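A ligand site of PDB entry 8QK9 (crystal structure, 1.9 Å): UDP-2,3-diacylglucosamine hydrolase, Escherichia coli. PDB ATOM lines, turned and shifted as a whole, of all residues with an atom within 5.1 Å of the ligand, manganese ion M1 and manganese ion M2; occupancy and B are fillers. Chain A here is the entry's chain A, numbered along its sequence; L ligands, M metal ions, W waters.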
ATOM      1  N   ASP A   8       0.279 -10.486  16.414  1.00  0.00           N
ATOM      2  CA  ASP A   8       0.012  -9.933  15.085  1.00  0.00           C
ATOM      3  C   ASP A   8       0.264 -10.968  14.009  1.00  0.00           C
ATOM      4  O   ASP A   8       0.846 -10.607  12.976  1.00  0.00           O
ATOM      5  CB  ASP A   8       0.854  -8.672  14.862  1.00  0.00           C
ATOM      6  CG  ASP A   8       0.431  -7.574  15.821  1.00  0.00           C
ATOM      7  OD1 ASP A   8      -0.727  -7.176  15.751  1.00  0.00           O
ATOM      8  OD2 ASP A   8       1.243  -7.184  16.658  1.00  0.00           O
ATOM      9  N   HIS A  10      -2.328 -12.488  12.508  1.00  0.00           N
ATOM     10  CA  HIS A  10      -3.423 -12.235  11.575  1.00  0.00           C
ATOM     11  C   HIS A  10      -3.746 -13.472  10.747  1.00  0.00           C
ATOM     12  O   HIS A  10      -3.884 -13.389   9.527  1.00  0.00           O
ATOM     13  CB  HIS A  10      -3.121 -11.022  10.673  1.00  0.00           C
ATOM     14  CG  HIS A  10      -3.115  -9.732  11.416  1.00  0.00           C
ATOM     15  ND1 HIS A  10      -4.200  -8.882  11.405  1.00  0.00           N
ATOM     16  CD2 HIS A  10      -2.188  -9.131  12.202  1.00  0.00           C
ATOM     17  CE1 HIS A  10      -3.941  -7.815  12.161  1.00  0.00           C
ATOM     18  NE2 HIS A  10      -2.730  -7.970  12.679  1.00  0.00           N
ATOM     19  N   ASP A  41      -4.265 -10.214  18.140  1.00  0.00           N
ATOM     20  CA  ASP A  41      -4.245 -10.318  16.693  1.00  0.00           C
ATOM     21  C   ASP A  41      -3.624 -11.619  16.246  1.00  0.00           C
ATOM     22  O   ASP A  41      -2.911 -11.641  15.235  1.00  0.00           O
ATOM     23  CB  ASP A  41      -3.569  -9.136  16.024  1.00  0.00           C
ATOM     24  CG  ASP A  41      -4.318  -7.811  16.165  1.00  0.00           C
ATOM     25  OD1 ASP A  41      -5.416  -7.837  16.808  1.00  0.00           O
ATOM     26  OD2 ASP A  41      -3.768  -6.763  15.672  1.00  0.00           O
ATOM     27  N   GLU A  44      -6.938 -12.772  11.917  1.00  0.00           N
ATOM     28  CA  GLU A  44      -7.257 -11.608  11.115  1.00  0.00           C
ATOM     29  C   GLU A  44      -8.582 -10.979  11.575  1.00  0.00           C
ATOM     30  O   GLU A  44      -8.784  -9.771  11.475  1.00  0.00           O
ATOM     31  CB  GLU A  44      -7.260 -12.014   9.627  1.00  0.00           C
ATOM     32  CG  GLU A  44      -7.631 -10.931   8.647  1.00  0.00           C
ATOM     33  CD  GLU A  44      -7.020  -9.567   8.878  1.00  0.00           C
ATOM     34  OE1 GLU A  44      -5.822  -9.481   9.233  1.00  0.00           O
ATOM     35  OE2 GLU A  44      -7.752  -8.577   8.701  1.00  0.00           O
ATOM     36  N   ALA A  45      -9.494 -11.824  12.088  1.00  0.00           N
ATOM     37  CA  ALA A  45     -10.841 -11.403  12.451  1.00  0.00           C
ATOM     38  C   ALA A  45     -11.444 -12.463  13.387  1.00  0.00           C
ATOM     39  O   ALA A  45     -10.988 -13.603  13.387  1.00  0.00           O
ATOM     40  CB  ALA A  45     -11.674 -11.214  11.203  1.00  0.00           C
ATOM     41  N   TRP A  46     -12.385 -12.075  14.247  1.00  0.00           N
ATOM     42  CA  TRP A  46     -13.096 -13.028  15.085  1.00  0.00           C
ATOM     43  C   TRP A  46     -14.532 -12.552  15.262  1.00  0.00           C
ATOM     44  O   TRP A  46     -14.765 -11.429  15.755  1.00  0.00           O
ATOM     45  CB  TRP A  46     -12.430 -13.185  16.445  1.00  0.00           C
ATOM     46  CG  TRP A  46     -12.826 -14.445  17.152  1.00  0.00           C
ATOM     47  CD1 TRP A  46     -13.776 -14.628  18.120  1.00  0.00           C
ATOM     48  CD2 TRP A  46     -12.210 -15.726  16.952  1.00  0.00           C
ATOM     49  NE1 TRP A  46     -13.814 -15.933  18.509  1.00  0.00           N
ATOM     50  CE2 TRP A  46     -12.847 -16.631  17.831  1.00  0.00           C
ATOM     51  CE3 TRP A  46     -11.206 -16.192  16.091  1.00  0.00           C
ATOM     52  CZ2 TRP A  46     -12.474 -17.981  17.894  1.00  0.00           C
ATOM     53  CZ3 TRP A  46     -10.862 -17.533  16.144  1.00  0.00           C
ATOM     54  CH2 TRP A  46     -11.480 -18.405  17.040  1.00  0.00           C
ATOM     55  N   ILE A  47     -15.499 -13.399  14.860  1.00  0.00           N
ATOM     56  CA  ILE A  47     -16.900 -13.025  14.979  1.00  0.00           C
ATOM     57  C   ILE A  47     -17.603 -13.908  16.002  1.00  0.00           C
ATOM     58  O   ILE A  47     -18.835 -13.849  16.116  1.00  0.00           O
ATOM     59  CB  ILE A  47     -17.633 -13.054  13.637  1.00  0.00           C
ATOM     60  CG1 ILE A  47     -17.558 -14.430  12.974  1.00  0.00           C
ATOM     61  CG2 ILE A  47     -17.140 -11.941  12.736  1.00  0.00           C
ATOM     62  CD1 ILE A  47     -18.400 -14.564  11.732  1.00  0.00           C
ATOM     63  N   GLY A  78      -6.307  -8.730  20.937  1.00  0.00           N
ATOM     64  CA  GLY A  78      -6.021  -7.579  20.115  1.00  0.00           C
ATOM     65  C   GLY A  78      -7.307  -6.906  19.620  1.00  0.00           C
ATOM     66  O   GLY A  78      -8.390  -7.321  20.016  1.00  0.00           O
ATOM     67  N   ASN A  79      -7.173  -5.907  18.747  1.00  0.00           N
ATOM     68  CA  ASN A  79      -8.320  -5.214  18.179  1.00  0.00           C
ATOM     69  C   ASN A  79      -9.040  -6.097  17.152  1.00  0.00           C
ATOM     70  O   ASN A  79     -10.218  -5.898  16.876  1.00  0.00           O
ATOM     71  CB  ASN A  79      -7.932  -3.863  17.558  1.00  0.00           C
ATOM     72  CG  ASN A  79      -6.891  -3.975  16.473  1.00  0.00           C
ATOM     73  OD1 ASN A  79      -5.768  -4.394  16.772  1.00  0.00           O
ATOM     74  ND2 ASN A  79      -7.194  -3.606  15.235  1.00  0.00           N
ATOM     75  N   ARG A  80      -8.329  -7.036  16.545  1.00  0.00           N
ATOM     76  CA  ARG A  80      -8.944  -7.913  15.573  1.00  0.00           C
ATOM     77  C   ARG A  80      -9.739  -9.034  16.238  1.00  0.00           C
ATOM     78  O   ARG A  80     -10.731  -9.489  15.667  1.00  0.00           O
ATOM     79  CB  ARG A  80      -7.920  -8.545  14.615  1.00  0.00           C
ATOM     80  CG  ARG A  80      -7.041  -7.540  13.893  1.00  0.00           C
ATOM     81  CD  ARG A  80      -7.829  -6.437  13.215  1.00  0.00           C
ATOM     82  NE  ARG A  80      -8.498  -6.952  12.048  1.00  0.00           N
ATOM     83  CZ  ARG A  80      -9.113  -6.227  11.131  1.00  0.00           C
ATOM     84  NH1 ARG A  80      -9.175  -4.915  11.256  1.00  0.00           N
ATOM     85  NH2 ARG A  80      -9.668  -6.825  10.096  1.00  0.00           N
ATOM     86  N   PHE A  82     -10.856  -9.382  19.738  1.00  0.00           N
ATOM     87  CA  PHE A  82     -11.329  -9.104  21.086  1.00  0.00           C
ATOM     88  C   PHE A  82     -12.521  -9.998  21.448  1.00  0.00           C
ATOM     89  O   PHE A  82     -12.819 -10.173  22.625  1.00  0.00           O
ATOM     90  CB  PHE A  82     -11.645  -7.615  21.282  1.00  0.00           C
ATOM     91  CG  PHE A  82     -12.710  -7.081  20.366  1.00  0.00           C
ATOM     92  CD1 PHE A  82     -12.389  -6.606  19.118  1.00  0.00           C
ATOM     93  CD2 PHE A  82     -14.050  -7.165  20.736  1.00  0.00           C
ATOM     94  CE1 PHE A  82     -13.375  -6.171  18.240  1.00  0.00           C
ATOM     95  CE2 PHE A  82     -15.031  -6.752  19.854  1.00  0.00           C
ATOM     96  CZ  PHE A  82     -14.693  -6.251  18.612  1.00  0.00           C
ATOM     97  N   LEU A  83     -13.230 -10.553  20.445  1.00  0.00           N
ATOM     98  CA  LEU A  83     -14.349 -11.440  20.781  1.00  0.00           C
ATOM     99  C   LEU A  83     -13.902 -12.865  21.108  1.00  0.00           C
ATOM    100  O   LEU A  83     -14.730 -13.666  21.490  1.00  0.00           O
ATOM    101  CB  LEU A  83     -15.366 -11.450  19.624  1.00  0.00           C
ATOM    102  CG  LEU A  83     -16.238 -10.198  19.465  1.00  0.00           C
ATOM    103  CD1 LEU A  83     -17.205 -10.341  18.277  1.00  0.00           C
ATOM    104  CD2 LEU A  83     -17.018  -9.914  20.740  1.00  0.00           C
ATOM    105  N   HIS A 114      -1.345  -5.720  24.189  1.00  0.00           N
ATOM    106  CA  HIS A 114      -1.428  -5.787  22.734  1.00  0.00           C
ATOM    107  C   HIS A 114      -0.755  -4.538  22.167  1.00  0.00           C
ATOM    108  O   HIS A 114       0.044  -4.625  21.229  1.00  0.00           O
ATOM    109  CB  HIS A 114      -2.878  -5.888  22.234  1.00  0.00           C
ATOM    110  CG  HIS A 114      -2.927  -5.981  20.756  1.00  0.00           C
ATOM    111  ND1 HIS A 114      -2.265  -6.950  20.031  1.00  0.00           N
ATOM    112  CD2 HIS A 114      -3.490  -5.175  19.844  1.00  0.00           C
ATOM    113  CE1 HIS A 114      -2.457  -6.711  18.714  1.00  0.00           C
ATOM    114  NE2 HIS A 114      -3.210  -5.643  18.600  1.00  0.00           N
ATOM    115  N   ASP A 122      -5.592   8.240  18.383  1.00  0.00           N
ATOM    116  CA  ASP A 122      -6.426   7.809  17.274  1.00  0.00           C
ATOM    117  C   ASP A 122      -7.869   7.806  17.745  1.00  0.00           C
ATOM    118  O   ASP A 122      -8.322   6.853  18.390  1.00  0.00           O
ATOM    119  CB  ASP A 122      -5.997   6.444  16.748  1.00  0.00           C
ATOM    120  CG  ASP A 122      -6.805   5.992  15.545  1.00  0.00           C
ATOM    121  OD1 ASP A 122      -7.910   6.563  15.304  1.00  0.00           O
ATOM    122  OD2 ASP A 122      -6.312   5.088  14.865  1.00  0.00           O
ATOM    123  N   GLY A 124     -10.947   7.926  16.236  1.00  0.00           N
ATOM    124  CA  GLY A 124     -11.826   6.936  15.630  1.00  0.00           C
ATOM    125  C   GLY A 124     -11.612   5.563  16.231  1.00  0.00           C
ATOM    126  O   GLY A 124     -12.556   4.916  16.675  1.00  0.00           O
ATOM    127  N   TYR A 125     -10.350   5.125  16.318  1.00  0.00           N
ATOM    128  CA  TYR A 125     -10.097   3.828  16.903  1.00  0.00           C
ATOM    129  C   TYR A 125     -10.570   3.814  18.363  1.00  0.00           C
ATOM    130  O   TYR A 125     -11.259   2.872  18.758  1.00  0.00           O
ATOM    131  CB  TYR A 125      -8.667   3.324  16.712  1.00  0.00           C
ATOM    132  CG  TYR A 125      -8.508   2.016  17.433  1.00  0.00           C
ATOM    133  CD1 TYR A 125      -9.109   0.863  16.943  1.00  0.00           C
ATOM    134  CD2 TYR A 125      -7.982   2.002  18.719  1.00  0.00           C
ATOM    135  CE1 TYR A 125      -9.090  -0.306  17.671  1.00  0.00           C
ATOM    136  CE2 TYR A 125      -7.932   0.833  19.459  1.00  0.00           C
ATOM    137  CZ  TYR A 125      -8.492  -0.322  18.919  1.00  0.00           C
ATOM    138  OH  TYR A 125      -8.434  -1.454  19.676  1.00  0.00           O
ATOM    139  N   PHE A 128     -14.468   3.563  18.465  1.00  0.00           N
ATOM    140  CA  PHE A 128     -14.733   2.184  18.062  1.00  0.00           C
ATOM    141  C   PHE A 128     -14.524   1.233  19.240  1.00  0.00           C
ATOM    142  O   PHE A 128     -15.425   0.474  19.606  1.00  0.00           O
ATOM    143  CB  PHE A 128     -13.855   1.793  16.894  1.00  0.00           C
ATOM    144  CG  PHE A 128     -13.921   0.342  16.497  1.00  0.00           C
ATOM    145  CD1 PHE A 128     -14.918  -0.125  15.649  1.00  0.00           C
ATOM    146  CD2 PHE A 128     -12.995  -0.574  16.988  1.00  0.00           C
ATOM    147  CE1 PHE A 128     -14.985  -1.456  15.282  1.00  0.00           C
ATOM    148  CE2 PHE A 128     -13.075  -1.913  16.629  1.00  0.00           C
ATOM    149  CZ  PHE A 128     -14.084  -2.349  15.797  1.00  0.00           C
ATOM    150  N   LYS A 131     -17.055   1.256  22.413  1.00  0.00           N
ATOM    151  CA  LYS A 131     -18.335   0.594  22.182  1.00  0.00           C
ATOM    152  C   LYS A 131     -18.184  -0.940  22.236  1.00  0.00           C
ATOM    153  O   LYS A 131     -18.827  -1.625  23.060  1.00  0.00           O
ATOM    154  CB  LYS A 131     -18.976   0.932  20.823  1.00  0.00           C
ATOM    155  CG  LYS A 131     -18.555   2.210  20.099  1.00  0.00           C
ATOM    156  CD  LYS A 131     -18.645   3.527  20.884  1.00  0.00           C
ATOM    157  CE  LYS A 131     -20.057   4.060  21.061  1.00  0.00           C
ATOM    158  NZ  LYS A 131     -20.798   3.311  22.094  1.00  0.00           N
ATOM    159  N   VAL A 132     -17.289  -1.472  21.370  1.00  0.00           N
ATOM    160  CA  VAL A 132     -17.248  -2.906  21.081  1.00  0.00           C
ATOM    161  C   VAL A 132     -16.715  -3.673  22.292  1.00  0.00           C
ATOM    162  O   VAL A 132     -16.825  -4.895  22.317  1.00  0.00           O
ATOM    163  CB  VAL A 132     -16.480  -3.239  19.797  1.00  0.00           C
ATOM    164  CG1 VAL A 132     -17.123  -2.580  18.583  1.00  0.00           C
ATOM    165  CG2 VAL A 132     -15.000  -2.888  19.852  1.00  0.00           C
ATOM    166  N   HIS A 133     -16.202  -2.956  23.304  1.00  0.00           N
ATOM    167  CA  HIS A 133     -15.733  -3.612  24.512  1.00  0.00           C
ATOM    168  C   HIS A 133     -16.797  -3.674  25.607  1.00  0.00           C
ATOM    169  O   HIS A 133     -16.548  -4.257  26.655  1.00  0.00           O
ATOM    170  CB  HIS A 133     -14.464  -2.958  25.045  1.00  0.00           C
ATOM    171  CG  HIS A 133     -13.237  -3.648  24.541  1.00  0.00           C
ATOM    172  ND1 HIS A 133     -12.806  -3.598  23.227  1.00  0.00           N
ATOM    173  CD2 HIS A 133     -12.392  -4.438  25.203  1.00  0.00           C
ATOM    174  CE1 HIS A 133     -11.710  -4.323  23.108  1.00  0.00           C
ATOM    175  NE2 HIS A 133     -11.432  -4.834  24.301  1.00  0.00           N
ATOM    176  N   LEU A 137     -23.144  -5.289  24.604  1.00  0.00           N
ATOM    177  CA  LEU A 137     -23.221  -5.123  23.178  1.00  0.00           C
ATOM    178  C   LEU A 137     -22.587  -6.329  22.473  1.00  0.00           C
ATOM    179  O   LEU A 137     -23.041  -6.727  21.405  1.00  0.00           O
ATOM    180  CB  LEU A 137     -22.450  -3.856  22.790  1.00  0.00           C
ATOM    181  CG  LEU A 137     -22.448  -3.582  21.294  1.00  0.00           C
ATOM    182  CD1 LEU A 137     -23.872  -3.537  20.759  1.00  0.00           C
ATOM    183  CD2 LEU A 137     -21.715  -2.298  20.979  1.00  0.00           C
ATOM    184  N   GLN A 138     -21.523  -6.860  23.075  1.00  0.00           N
ATOM    185  CA  GLN A 138     -20.880  -8.073  22.572  1.00  0.00           C
ATOM    186  C   GLN A 138     -21.898  -9.213  22.596  1.00  0.00           C
ATOM    187  O   GLN A 138     -22.002  -9.984  21.662  1.00  0.00           O
ATOM    188  CB  GLN A 138     -19.622  -8.410  23.397  1.00  0.00           C
ATOM    189  CG  GLN A 138     -18.453  -7.448  23.217  1.00  0.00           C
ATOM    190  CD  GLN A 138     -17.246  -7.825  24.043  1.00  0.00           C
ATOM    191  OE1 GLN A 138     -17.318  -8.699  24.889  1.00  0.00           O
ATOM    192  NE2 GLN A 138     -16.121  -7.160  23.833  1.00  0.00           N
ATOM    193  N   PHE A 141     -24.330  -8.880  19.615  1.00  0.00           N
ATOM    194  CA  PHE A 141     -23.698  -9.222  18.345  1.00  0.00           C
ATOM    195  C   PHE A 141     -23.545 -10.748  18.238  1.00  0.00           C
ATOM    196  O   PHE A 141     -23.796 -11.322  17.168  1.00  0.00           O
ATOM    197  CB  PHE A 141     -22.359  -8.486  18.195  1.00  0.00           C
ATOM    198  CG  PHE A 141     -21.571  -8.863  16.955  1.00  0.00           C
ATOM    199  CD1 PHE A 141     -21.797  -8.227  15.754  1.00  0.00           C
ATOM    200  CD2 PHE A 141     -20.619  -9.875  17.006  1.00  0.00           C
ATOM    201  CE1 PHE A 141     -21.086  -8.583  14.626  1.00  0.00           C
ATOM    202  CE2 PHE A 141     -19.907 -10.231  15.878  1.00  0.00           C
ATOM    203  CZ  PHE A 141     -20.151  -9.583  14.688  1.00  0.00           C
ATOM    204  N   ILE A 152     -21.661  -8.209   8.477  1.00  0.00           N
ATOM    205  CA  ILE A 152     -21.279  -7.025   9.228  1.00  0.00           C
ATOM    206  C   ILE A 152     -19.761  -6.850   9.153  1.00  0.00           C
ATOM    207  O   ILE A 152     -19.263  -5.765   8.877  1.00  0.00           O
ATOM    208  CB  ILE A 152     -21.769  -7.108  10.686  1.00  0.00           C
ATOM    209  CG1 ILE A 152     -23.295  -6.983  10.790  1.00  0.00           C
ATOM    210  CG2 ILE A 152     -21.071  -6.063  11.537  1.00  0.00           C
ATOM    211  CD1 ILE A 152     -23.855  -7.301  12.146  1.00  0.00           C
ATOM    212  N   ALA A 153     -19.036  -7.949   9.424  1.00  0.00           N
ATOM    213  CA  ALA A 153     -17.582  -7.949   9.490  1.00  0.00           C
ATOM    214  C   ALA A 153     -16.935  -7.654   8.144  1.00  0.00           C
ATOM    215  O   ALA A 153     -15.837  -7.099   8.117  1.00  0.00           O
ATOM    216  CB  ALA A 153     -17.123  -9.291  10.035  1.00  0.00           C
ATOM    217  N   MET A 156     -17.014  -3.817   8.032  1.00  0.00           N
ATOM    218  CA  MET A 156     -16.173  -3.110   8.994  1.00  0.00           C
ATOM    219  C   MET A 156     -14.697  -3.140   8.600  1.00  0.00           C
ATOM    220  O   MET A 156     -13.910  -2.352   9.117  1.00  0.00           O
ATOM    221  CB  MET A 156     -16.275  -3.698  10.393  1.00  0.00           C
ATOM    222  CG  MET A 156     -17.658  -3.710  10.947  1.00  0.00           C
ATOM    223  SD  MET A 156     -17.564  -3.607  12.713  1.00  0.00           S
ATOM    224  CE  MET A 156     -17.954  -1.876  12.946  1.00  0.00           C
ATOM    225  N   ARG A 157     -14.328  -4.081   7.716  1.00  0.00           N
ATOM    226  CA  ARG A 157     -12.929  -4.296   7.359  1.00  0.00           C
ATOM    227  C   ARG A 157     -12.598  -3.573   6.052  1.00  0.00           C
ATOM    228  O   ARG A 157     -11.498  -3.013   5.934  1.00  0.00           O
ATOM    229  CB  ARG A 157     -12.646  -5.796   7.332  1.00  0.00           C
ATOM    230  CG  ARG A 157     -12.706  -6.423   8.717  1.00  0.00           C
ATOM    231  CD  ARG A 157     -12.164  -7.838   8.724  1.00  0.00           C
ATOM    232  NE  ARG A 157     -13.044  -8.787   8.065  1.00  0.00           N
ATOM    233  CZ  ARG A 157     -12.708 -10.034   7.778  1.00  0.00           C
ATOM    234  NH1 ARG A 157     -11.476 -10.466   7.997  1.00  0.00           N
ATOM    235  NH2 ARG A 157     -13.607 -10.855   7.251  1.00  0.00           N
ATOM    236  N   SER A 160     -12.227  -0.019   7.553  1.00  0.00           N
ATOM    237  CA  SER A 160     -10.827   0.004   7.976  1.00  0.00           C
ATOM    238  C   SER A 160      -9.939  -0.386   6.789  1.00  0.00           C
ATOM    239  O   SER A 160      -8.884   0.246   6.621  1.00  0.00           O
ATOM    240  CB  SER A 160     -10.571  -0.919   9.161  1.00  0.00           C
ATOM    241  OG  SER A 160     -11.269  -0.510  10.329  1.00  0.00           O
ATOM    242  N   ALA A 170      -2.208   0.834   7.465  1.00  0.00           N
ATOM    243  CA  ALA A 170      -2.091   2.151   8.136  1.00  0.00           C
ATOM    244  C   ALA A 170      -2.650   2.042   9.547  1.00  0.00           C
ATOM    245  O   ALA A 170      -3.860   2.150   9.772  1.00  0.00           O
ATOM    246  CB  ALA A 170      -2.801   3.198   7.309  1.00  0.00           C
ATOM    247  N   ILE A 171      -1.756   1.772  10.510  1.00  0.00           N
ATOM    248  CA  ILE A 171      -2.092   1.690  11.924  1.00  0.00           C
ATOM    249  C   ILE A 171      -1.342   2.818  12.649  1.00  0.00           C
ATOM    250  O   ILE A 171      -0.121   2.920  12.521  1.00  0.00           O
ATOM    251  CB  ILE A 171      -1.728   0.298  12.477  1.00  0.00           C
ATOM    252  CG1 ILE A 171      -2.583  -0.800  11.854  1.00  0.00           C
ATOM    253  CG2 ILE A 171      -1.791   0.274  14.002  1.00  0.00           C
ATOM    254  CD1 ILE A 171      -2.031  -2.178  12.061  1.00  0.00           C
ATOM    255  N   HIS A 195       0.599  -4.712  17.858  1.00  0.00           N
ATOM    256  CA  HIS A 195      -0.420  -3.837  17.315  1.00  0.00           C
ATOM    257  C   HIS A 195       0.090  -2.939  16.186  1.00  0.00           C
ATOM    258  O   HIS A 195      -0.586  -2.788  15.171  1.00  0.00           O
ATOM    259  CB  HIS A 195      -1.000  -2.917  18.380  1.00  0.00           C
ATOM    260  CG  HIS A 195      -2.078  -2.027  17.838  1.00  0.00           C
ATOM    261  ND1 HIS A 195      -3.223  -2.474  17.201  1.00  0.00           N
ATOM    262  CD2 HIS A 195      -2.135  -0.692  17.764  1.00  0.00           C
ATOM    263  CE1 HIS A 195      -3.953  -1.436  16.809  1.00  0.00           C
ATOM    264  NE2 HIS A 195      -3.316  -0.338  17.149  1.00  0.00           N
ATOM    265  N   HIS A 197       2.786  -3.018  14.279  1.00  0.00           N
ATOM    266  CA  HIS A 197       3.475  -3.630  13.148  1.00  0.00           C
ATOM    267  C   HIS A 197       4.768  -2.866  12.788  1.00  0.00           C
ATOM    268  O   HIS A 197       5.196  -2.831  11.623  1.00  0.00           O
ATOM    269  CB  HIS A 197       2.550  -3.765  11.913  1.00  0.00           C
ATOM    270  CG  HIS A 197       1.284  -4.538  12.110  1.00  0.00           C
ATOM    271  ND1 HIS A 197       0.358  -4.765  11.103  1.00  0.00           N
ATOM    272  CD2 HIS A 197       0.766  -5.098  13.234  1.00  0.00           C
ATOM    273  CE1 HIS A 197      -0.678  -5.450  11.597  1.00  0.00           C
ATOM    274  NE2 HIS A 197      -0.459  -5.662  12.900  1.00  0.00           N
HETATM  275  C1  LIG L   1     -17.462  -7.237  13.632  1.00  0.00           C
HETATM  276  C2  LIG L   1     -16.084  -6.997  13.035  1.00  0.00           C
HETATM  277  C3  LIG L   1     -19.987  -4.389  15.908  1.00  0.00           C
HETATM  278  C4  LIG L   1     -19.017  -5.112  15.185  1.00  0.00           C
HETATM  279  C5  LIG L   1     -18.306  -6.190  15.773  1.00  0.00           C
HETATM  280  C6  LIG L   1     -18.549  -6.477  17.095  1.00  0.00           C
HETATM  281  C7  LIG L   1     -19.475  -5.742  17.801  1.00  0.00           C
HETATM  282  C8  LIG L   1     -20.221  -4.719  17.223  1.00  0.00           C
HETATM  283  N1  LIG L   1     -17.250  -6.904  15.055  1.00  0.00           N
HETATM  284  C9  LIG L   1     -16.461  -7.958  15.752  1.00  0.00           C
HETATM  285  C10 LIG L   1     -15.065  -7.975  15.103  1.00  0.00           C
HETATM  286  N2  LIG L   1     -15.191  -8.046  13.615  1.00  0.00           N
HETATM  287  S1  LIG L   1     -13.733  -8.061  12.867  1.00  0.00           S
HETATM  288  C11 LIG L   1     -12.975  -6.482  12.978  1.00  0.00           C
HETATM  289  O1  LIG L   1     -12.900  -9.066  13.523  1.00  0.00           O
HETATM  290  O2  LIG L   1     -13.904  -8.353  11.452  1.00  0.00           O
HETATM  291  C12 LIG L   1     -13.315  -5.522  11.999  1.00  0.00           C
HETATM  292  C13 LIG L   1     -12.780  -4.255  12.059  1.00  0.00           C
HETATM  293  C14 LIG L   1     -11.861  -3.931  13.062  1.00  0.00           C
HETATM  294  C15 LIG L   1     -12.108  -6.162  14.019  1.00  0.00           C
HETATM  295  C16 LIG L   1     -11.560  -4.884  14.061  1.00  0.00           C
HETATM  296  N3  LIG L   1     -11.400  -2.588  13.091  1.00  0.00           N
HETATM  297  C17 LIG L   1     -10.427  -2.051  13.878  1.00  0.00           C
HETATM  298  O3  LIG L   1      -9.707  -2.764  14.578  1.00  0.00           O
HETATM  299  C18 LIG L   1     -10.214  -0.544  13.753  1.00  0.00           C
HETATM  300  C19 LIG L   1     -11.353   0.299  13.799  1.00  0.00           C
HETATM  301  C20 LIG L   1     -11.231   1.691  13.620  1.00  0.00           C
HETATM  302  C21 LIG L   1      -9.994   2.268  13.389  1.00  0.00           C
HETATM  303  C22 LIG L   1      -8.840   1.447  13.317  1.00  0.00           C
HETATM  304  C23 LIG L   1      -8.948   0.029  13.502  1.00  0.00           C
HETATM  305  N4  LIG L   1      -7.750  -0.866  13.429  1.00  0.00           N
HETATM  306  C24 LIG L   1      -6.502  -0.342  14.072  1.00  0.00           C
HETATM  307  S2  LIG L   1      -7.452  -1.468  11.909  1.00  0.00           S
HETATM  308  C25 LIG L   1      -6.747  -0.206  10.869  1.00  0.00           C
HETATM  309  O4  LIG L   1      -6.598  -2.586  12.050  1.00  0.00           O
HETATM  310  O5  LIG L   1      -8.700  -1.957  11.363  1.00  0.00           O
HETATM  311  C26 LIG L   1     -19.706  -6.147  19.237  1.00  0.00           C
HETATM  312  F1  LIG L   1     -21.032  -6.051  19.516  1.00  0.00           F
HETATM  313  F2  LIG L   1     -19.267  -7.397  19.410  1.00  0.00           F
HETATM  314  F3  LIG L   1     -19.000  -5.396  20.079  1.00  0.00           F
HETATM  315 MN    MN M   1      -3.741  -4.776  16.583  1.00  0.00          MN
HETATM  316 MN    MN M   2      -2.052  -6.480  14.233  1.00  0.00          MN
HETATM  317  O   HOH W   1      -2.696  -4.450  14.730  1.00  0.00           O
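An oxygen (O3) of the ligand lies within hydrogen-bond range of the side-chain amide nitrogen (ND2) of Asn 79 (2.7 Å).
O5 of the ligand lies within hydrogen-bond range of NH1 of Arg 80 (3.0 Å).
The side-chain hydroxyl (OG) of Ser 160 sits close to an oxygen (O5) of the ligand, 3.1 Å away.
An oxygen (O1) of the ligand is in hydrogen-bond range of the backbone NH of Trp 46, at 3.1 Å.
OD2 of Asp 8 lies within hydrogen-bond range of N of His 195.
The side-chain carboxylate (OD1) of Asp 41 is in hydrogen-bond range of the backbone NH (N) of Arg 80.
The side-chain carboxylate of Glu 44 is in hydrogen-bond range of a ring nitrogen (ND1) of His 10 (2.8 Å).
N of Trp 46 lies within hydrogen-bond range of O of Arg 80 (3.4 Å).
The side-chain carboxylate (OE2) of Glu 44 is in salt-bridge range of the guanidinium group (NH2) of Arg 80, at 2.9 Å.
The backbone carbonyl oxygen (O) of Val 132 lies within hydrogen-bond range of the side-chain amide nitrogen (NE2) of Gln 138, 2.8 Å away.
The backbone carbonyl oxygen of Ala 153 lies close to the guanidinium group of Arg 157 (3.3 Å).
The backbone NH of Tyr 125 sits at hydrogen-bond distance from the side-chain carboxylate of Asp 122 (3.0 Å).
The backbone carbonyl oxygen (O) of Val 132 sits close to a fluorine (F3) of the ligand, at 3.2 Å.
F1 of the ligand lies close to O of Leu 137.
Residues that only touch the ligand: Phe 141, Met 156, Arg 157, Ala 45, Tyr 125, Leu 83, Gln 138, Ala 153, Phe 128, Phe 82 and Ala 170.
Hydrophobic or aromatic side chains that line the ligand: Ala 45, Phe 82, Leu 83, Tyr 125, Phe 128, Val 132, Leu 137, Phe 141, Ala 153, Met 156 and His 195.
Of the 32 residues printed, 18 come within 4 Å of the ligand.
The nearest printed residue that does not touch the ligand is Ile 152 (4.3 Å).
Of the 32 residues printed, 4 come within 4 Å of manganese ion M2.
Manganese ion M1 is bound by OD1 of Asn 79 (2.1 Å), water W1 (2.2 Å), OD2 of Asp 41 (2.2 Å), NE2 of His 114 (2.3 Å) and ND1 of His 195 (2.4 Å).
The side-chain carboxylate (OD1) of Asp 8 binds manganese ion M2, at 2.1 Å.
Water W1 is bound to manganese ion M2.
NE2 of His 197 is bound to manganese ion M2.
NE2 of His 10 binds manganese ion M2 (2.3 Å).
OD2 of Asp 41 binds manganese ion M2, at 2.3 Å.
Manganese ion M2 has five donor atoms within binding distance.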
